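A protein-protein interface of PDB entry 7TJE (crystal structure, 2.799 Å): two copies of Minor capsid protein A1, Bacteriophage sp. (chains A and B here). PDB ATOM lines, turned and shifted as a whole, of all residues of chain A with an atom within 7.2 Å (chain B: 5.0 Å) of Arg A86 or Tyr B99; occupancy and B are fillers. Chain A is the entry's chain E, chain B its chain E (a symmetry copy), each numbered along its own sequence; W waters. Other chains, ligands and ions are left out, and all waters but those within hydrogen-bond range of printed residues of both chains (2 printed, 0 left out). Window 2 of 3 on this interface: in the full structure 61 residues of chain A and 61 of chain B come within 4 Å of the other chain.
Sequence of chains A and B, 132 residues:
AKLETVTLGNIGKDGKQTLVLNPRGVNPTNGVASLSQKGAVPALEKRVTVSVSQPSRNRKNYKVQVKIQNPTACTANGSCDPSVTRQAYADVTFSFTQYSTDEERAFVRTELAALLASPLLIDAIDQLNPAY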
ATOM      1  N   ASN A  70     -24.073  -4.068   2.395  1.00  0.00           N
ATOM      2  CA  ASN A  70     -22.914  -4.218   3.259  1.00  0.00           C
ATOM      3  C   ASN A  70     -23.151  -3.460   4.547  1.00  0.00           C
ATOM      4  O   ASN A  70     -23.238  -2.226   4.509  1.00  0.00           O
ATOM      5  CB  ASN A  70     -21.662  -3.699   2.566  1.00  0.00           C
ATOM      6  CG  ASN A  70     -21.241  -4.568   1.427  1.00  0.00           C
ATOM      7  OD1 ASN A  70     -21.808  -5.643   1.213  1.00  0.00           O
ATOM      8  ND2 ASN A  70     -20.232  -4.119   0.684  1.00  0.00           N
ATOM      9  N   PRO A  71     -23.262  -4.125   5.697  1.00  0.00           N
ATOM     10  CA  PRO A  71     -23.490  -3.402   6.944  1.00  0.00           C
ATOM     11  C   PRO A  71     -22.173  -2.899   7.494  1.00  0.00           C
ATOM     12  O   PRO A  71     -21.105  -3.416   7.185  1.00  0.00           O
ATOM     13  CB  PRO A  71     -24.091  -4.471   7.867  1.00  0.00           C
ATOM     14  CG  PRO A  71     -24.156  -5.730   7.056  1.00  0.00           C
ATOM     15  CD  PRO A  71     -23.154  -5.564   5.968  1.00  0.00           C
ATOM     16  N   THR A  72     -22.265  -1.852   8.293  1.00  0.00           N
ATOM     17  CA  THR A  72     -21.164  -1.407   9.129  1.00  0.00           C
ATOM     18  C   THR A  72     -21.565  -1.634  10.578  1.00  0.00           C
ATOM     19  O   THR A  72     -22.677  -1.277  10.983  1.00  0.00           O
ATOM     20  CB  THR A  72     -20.839   0.071   8.906  1.00  0.00           C
ATOM     21  OG1 THR A  72     -20.317   0.270   7.586  1.00  0.00           O
ATOM     22  CG2 THR A  72     -19.817   0.532   9.928  1.00  0.00           C
ATOM     23  N   ALA A  73     -20.670  -2.228  11.351  1.00  0.00           N
ATOM     24  CA  ALA A  73     -20.928  -2.520  12.749  1.00  0.00           C
ATOM     25  C   ALA A  73     -20.007  -1.695  13.634  1.00  0.00           C
ATOM     26  O   ALA A  73     -18.894  -1.343  13.243  1.00  0.00           O
ATOM     27  CB  ALA A  73     -20.739  -4.011  13.044  1.00  0.00           C
ATOM     28  N   CYS A  74     -20.490  -1.381  14.829  1.00  0.00           N
ATOM     29  CA  CYS A  74     -19.684  -0.716  15.844  1.00  0.00           C
ATOM     30  C   CYS A  74     -19.893  -1.454  17.155  1.00  0.00           C
ATOM     31  O   CYS A  74     -21.025  -1.531  17.650  1.00  0.00           O
ATOM     32  CB  CYS A  74     -20.055   0.763  15.971  1.00  0.00           C
ATOM     33  SG  CYS A  74     -19.440   1.605  17.461  1.00  0.00           S
ATOM     34  N   SER A  83     -23.278  -3.691  16.876  1.00  0.00           N
ATOM     35  CA  SER A  83     -24.559  -3.379  16.252  1.00  0.00           C
ATOM     36  C   SER A  83     -24.357  -2.774  14.868  1.00  0.00           C
ATOM     37  O   SER A  83     -23.353  -2.109  14.611  1.00  0.00           O
ATOM     38  CB  SER A  83     -25.373  -2.413  17.110  1.00  0.00           C
ATOM     39  OG  SER A  83     -25.706  -3.032  18.333  1.00  0.00           O
ATOM     40  N   VAL A  84     -25.314  -3.011  13.975  1.00  0.00           N
ATOM     41  CA  VAL A  84     -25.295  -2.393  12.649  1.00  0.00           C
ATOM     42  C   VAL A  84     -25.699  -0.932  12.804  1.00  0.00           C
ATOM     43  O   VAL A  84     -26.761  -0.629  13.363  1.00  0.00           O
ATOM     44  CB  VAL A  84     -26.225  -3.130  11.670  1.00  0.00           C
ATOM     45  CG1 VAL A  84     -26.421  -2.349  10.375  1.00  0.00           C
ATOM     46  CG2 VAL A  84     -25.687  -4.499  11.358  1.00  0.00           C
ATOM     47  N   THR A  85     -24.842  -0.020  12.323  1.00  0.00           N
ATOM     48  CA  THR A  85     -25.114   1.409  12.391  1.00  0.00           C
ATOM     49  C   THR A  85     -25.396   2.065  11.044  1.00  0.00           C
ATOM     50  O   THR A  85     -25.864   3.203  11.035  1.00  0.00           O
ATOM     51  CB  THR A  85     -23.953   2.161  13.069  1.00  0.00           C
ATOM     52  OG1 THR A  85     -22.735   1.987  12.326  1.00  0.00           O
ATOM     53  CG2 THR A  85     -23.748   1.670  14.496  1.00  0.00           C
ATOM     54  N   ARG A  86     -25.113   1.405   9.921  1.00  0.00           N
ATOM     55  CA  ARG A  86     -25.567   1.866   8.609  1.00  0.00           C
ATOM     56  C   ARG A  86     -25.451   0.712   7.623  1.00  0.00           C
ATOM     57  O   ARG A  86     -24.753  -0.273   7.863  1.00  0.00           O
ATOM     58  CB  ARG A  86     -24.762   3.064   8.092  1.00  0.00           C
ATOM     59  CG  ARG A  86     -23.259   2.889   8.238  1.00  0.00           C
ATOM     60  CD  ARG A  86     -22.473   4.100   7.765  1.00  0.00           C
ATOM     61  NE  ARG A  86     -21.026   3.941   7.987  1.00  0.00           N
ATOM     62  CZ  ARG A  86     -20.397   4.265   9.119  1.00  0.00           C
ATOM     63  NH1 ARG A  86     -21.079   4.766  10.140  1.00  0.00           N
ATOM     64  NH2 ARG A  86     -19.087   4.089   9.233  1.00  0.00           N
ATOM     65  N   GLN A  87     -26.118   0.867   6.493  1.00  0.00           N
ATOM     66  CA  GLN A  87     -25.977  -0.048   5.378  1.00  0.00           C
ATOM     67  C   GLN A  87     -25.559   0.720   4.138  1.00  0.00           C
ATOM     68  O   GLN A  87     -26.062   1.814   3.870  1.00  0.00           O
ATOM     69  CB  GLN A  87     -27.287  -0.793   5.067  1.00  0.00           C
ATOM     70  CG  GLN A  87     -28.063  -1.300   6.260  1.00  0.00           C
ATOM     71  CD  GLN A  87     -27.690  -2.712   6.650  1.00  0.00           C
ATOM     72  OE1 GLN A  87     -26.718  -3.284   6.145  1.00  0.00           O
ATOM     73  NE2 GLN A  87     -28.446  -3.272   7.577  1.00  0.00           N
ATOM     74  N   ALA A  88     -24.662   0.125   3.373  1.00  0.00           N
ATOM     75  CA  ALA A  88     -24.405   0.510   1.995  1.00  0.00           C
ATOM     76  C   ALA A  88     -25.178  -0.417   1.057  1.00  0.00           C
ATOM     77  O   ALA A  88     -25.234  -1.629   1.280  1.00  0.00           O
ATOM     78  CB  ALA A  88     -22.908   0.436   1.699  1.00  0.00           C
ATOM     79  N   TYR A  89     -25.785   0.153   0.014  1.00  0.00           N
ATOM     80  CA  TYR A  89     -26.584  -0.623  -0.928  1.00  0.00           C
ATOM     81  C   TYR A  89     -26.171  -0.327  -2.357  1.00  0.00           C
ATOM     82  O   TYR A  89     -25.905   0.827  -2.722  1.00  0.00           O
ATOM     83  CB  TYR A  89     -28.085  -0.341  -0.835  1.00  0.00           C
ATOM     84  CG  TYR A  89     -28.731  -0.661   0.481  1.00  0.00           C
ATOM     85  CD1 TYR A  89     -29.149  -1.953   0.792  1.00  0.00           C
ATOM     86  CD2 TYR A  89     -28.943   0.339   1.420  1.00  0.00           C
ATOM     87  CE1 TYR A  89     -29.761  -2.233   2.013  1.00  0.00           C
ATOM     88  CE2 TYR A  89     -29.543   0.068   2.628  1.00  0.00           C
ATOM     89  CZ  TYR A  89     -29.961  -1.210   2.925  1.00  0.00           C
ATOM     90  OH  TYR A  89     -30.573  -1.426   4.147  1.00  0.00           O
ATOM     91  N   THR B  97     -25.390   6.182   3.412  1.00  0.00           N
ATOM     92  CA  THR B  97     -25.701   7.004   4.571  1.00  0.00           C
ATOM     93  C   THR B  97     -24.830   8.263   4.573  1.00  0.00           C
ATOM     94  O   THR B  97     -23.764   8.323   3.945  1.00  0.00           O
ATOM     95  CB  THR B  97     -25.526   6.145   5.837  1.00  0.00           C
ATOM     96  OG1 THR B  97     -26.696   5.341   6.006  1.00  0.00           O
ATOM     97  CG2 THR B  97     -25.283   6.917   7.112  1.00  0.00           C
ATOM     98  N   GLN B  98     -25.322   9.308   5.244  1.00  0.00           N
ATOM     99  CA  GLN B  98     -24.505  10.503   5.366  1.00  0.00           C
ATOM    100  C   GLN B  98     -23.268  10.270   6.224  1.00  0.00           C
ATOM    101  O   GLN B  98     -22.333  11.073   6.183  1.00  0.00           O
ATOM    102  CB  GLN B  98     -25.354  11.636   5.910  1.00  0.00           C
ATOM    103  CG  GLN B  98     -25.272  12.882   5.042  1.00  0.00           C
ATOM    104  CD  GLN B  98     -26.036  14.044   5.633  1.00  0.00           C
ATOM    105  OE1 GLN B  98     -26.832  13.851   6.561  1.00  0.00           O
ATOM    106  NE2 GLN B  98     -25.797  15.265   5.109  1.00  0.00           N
ATOM    107  N   TYR B  99     -23.208   9.163   6.950  1.00  0.00           N
ATOM    108  CA  TYR B  99     -22.074   8.846   7.797  1.00  0.00           C
ATOM    109  C   TYR B  99     -21.175   7.784   7.186  1.00  0.00           C
ATOM    110  O   TYR B  99     -20.255   7.317   7.858  1.00  0.00           O
ATOM    111  CB  TYR B  99     -22.551   8.409   9.180  1.00  0.00           C
ATOM    112  CG  TYR B  99     -23.082   9.547  10.019  1.00  0.00           C
ATOM    113  CD1 TYR B  99     -22.219  10.412  10.685  1.00  0.00           C
ATOM    114  CD2 TYR B  99     -24.451   9.763  10.145  1.00  0.00           C
ATOM    115  CE1 TYR B  99     -22.714  11.447  11.459  1.00  0.00           C
ATOM    116  CE2 TYR B  99     -24.945  10.788  10.903  1.00  0.00           C
ATOM    117  CZ  TYR B  99     -24.075  11.623  11.566  1.00  0.00           C
ATOM    118  OH  TYR B  99     -24.573  12.651  12.328  1.00  0.00           O
ATOM    119  N   SER B 100     -21.409   7.406   5.930  1.00  0.00           N
ATOM    120  CA  SER B 100     -20.569   6.430   5.252  1.00  0.00           C
ATOM    121  C   SER B 100     -19.233   7.043   4.876  1.00  0.00           C
ATOM    122  O   SER B 100     -19.084   8.256   4.796  1.00  0.00           O
ATOM    123  CB  SER B 100     -21.256   5.923   3.987  1.00  0.00           C
ATOM    124  OG  SER B 100     -21.225   6.931   2.981  1.00  0.00           O
ATOM    125  N   THR B 101     -18.271   6.184   4.586  1.00  0.00           N
ATOM    126  CA  THR B 101     -16.933   6.590   4.192  1.00  0.00           C
ATOM    127  C   THR B 101     -16.675   6.229   2.736  1.00  0.00           C
ATOM    128  O   THR B 101     -17.324   5.357   2.160  1.00  0.00           O
ATOM    129  CB  THR B 101     -15.881   5.910   5.069  1.00  0.00           C
ATOM    130  OG1 THR B 101     -15.764   4.539   4.673  1.00  0.00           O
ATOM    131  CG2 THR B 101     -16.279   5.989   6.545  1.00  0.00           C
ATOM    132  N   GLU B 104     -16.082   2.512   2.272  1.00  0.00           N
ATOM    133  CA  GLU B 104     -17.291   1.705   2.127  1.00  0.00           C
ATOM    134  C   GLU B 104     -17.936   1.913   0.756  1.00  0.00           C
ATOM    135  O   GLU B 104     -18.457   0.965   0.155  1.00  0.00           O
ATOM    136  CB  GLU B 104     -18.284   2.037   3.238  1.00  0.00           C
ATOM    137  CG  GLU B 104     -17.675   2.033   4.632  1.00  0.00           C
ATOM    138  CD  GLU B 104     -18.604   2.618   5.690  1.00  0.00           C
ATOM    139  OE1 GLU B 104     -19.599   3.300   5.313  1.00  0.00           O
ATOM    140  OE2 GLU B 104     -18.356   2.372   6.895  1.00  0.00           O
HETATM  141  O   HOH W   1     -28.410   2.667   6.924  1.00  0.00           O
HETATM  142  O   HOH W   2     -24.096   3.870   3.810  1.00  0.00           O
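NE of Arg A86 lies close to O of Tyr B99 (3.5 Å). The side-chain carboxylate of Glu B104 is in salt-bridge range of the guanidinium group of Arg A86. The side-chain carboxylate (OE2) of Glu B104 lies within hydrogen-bond range of the side-chain hydroxyl (OG1) of Thr A72, at 3.0 Å.
The backbone carbonyl oxygen of Thr A72 sits at hydrogen-bond distance from the backbone NH of Thr A85, 2.8 Å away. The side-chain hydroxyl (OG1) of Thr B101 sits close to the backbone NH (N) of Glu B104, 3.2 Å away. OG of Ser B100 lies within hydrogen-bond range of O of Thr B97, at 3.1 Å. The backbone NH of Thr A72 is in hydrogen-bond range of the backbone carbonyl oxygen of Arg A86, 3.0 Å away.
Among the printed residues, merely in contact across the chains: Arg A86 with Thr B97 and Arg A86 with Ser B100.
Arg A86 touches just these residues of chain B: Thr B97, Tyr B99, Ser B100 and Glu B104. Tyr B99 touches one residue of chain A. Of the printed residues of chain A, Ser B100 touches Arg A86 (3.7 Å). Of the printed residues of chain A, Thr B97 touches Arg A86 (3.6 Å). Of the printed residues of chain A, Glu B104 touches Thr A72 and Arg A86. Printed residues of chain B within 4 Å of Thr A72: Glu B104 (3.0 Å). Tyr A89 touches none of the printed residues of chain B. Gln A87 touches none of the printed residues of chain B. The nearest residue of chain A that does not touch Tyr B99 is Thr A85 (6.4 Å). The nearest printed residue of chain A that does not touch Glu B104 is Ala A88 (4.7 Å).
Of the 12 printed residues of chain A, 2 touch a printed residue of chain B. Among the printed residues, 5 pairs touch across the chains. Among the printed residues, Asp or Glu carboxylates within 4 Å of a Lys or Arg side-chain nitrogen of the other chain: Arg A86 with Glu B104 (3.0 Å).
No position is printed for both chains.
Water W2 bridges the backbone NH of Thr B97 (2.7 Å) and the backbone carbonyl oxygen of Gln A87 (2.8 Å). Water W1 bridges the backbone NH (N) of Gln A87 (2.9 Å) and the side-chain hydroxyl (OG1) of Thr B97 (3.3 Å).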
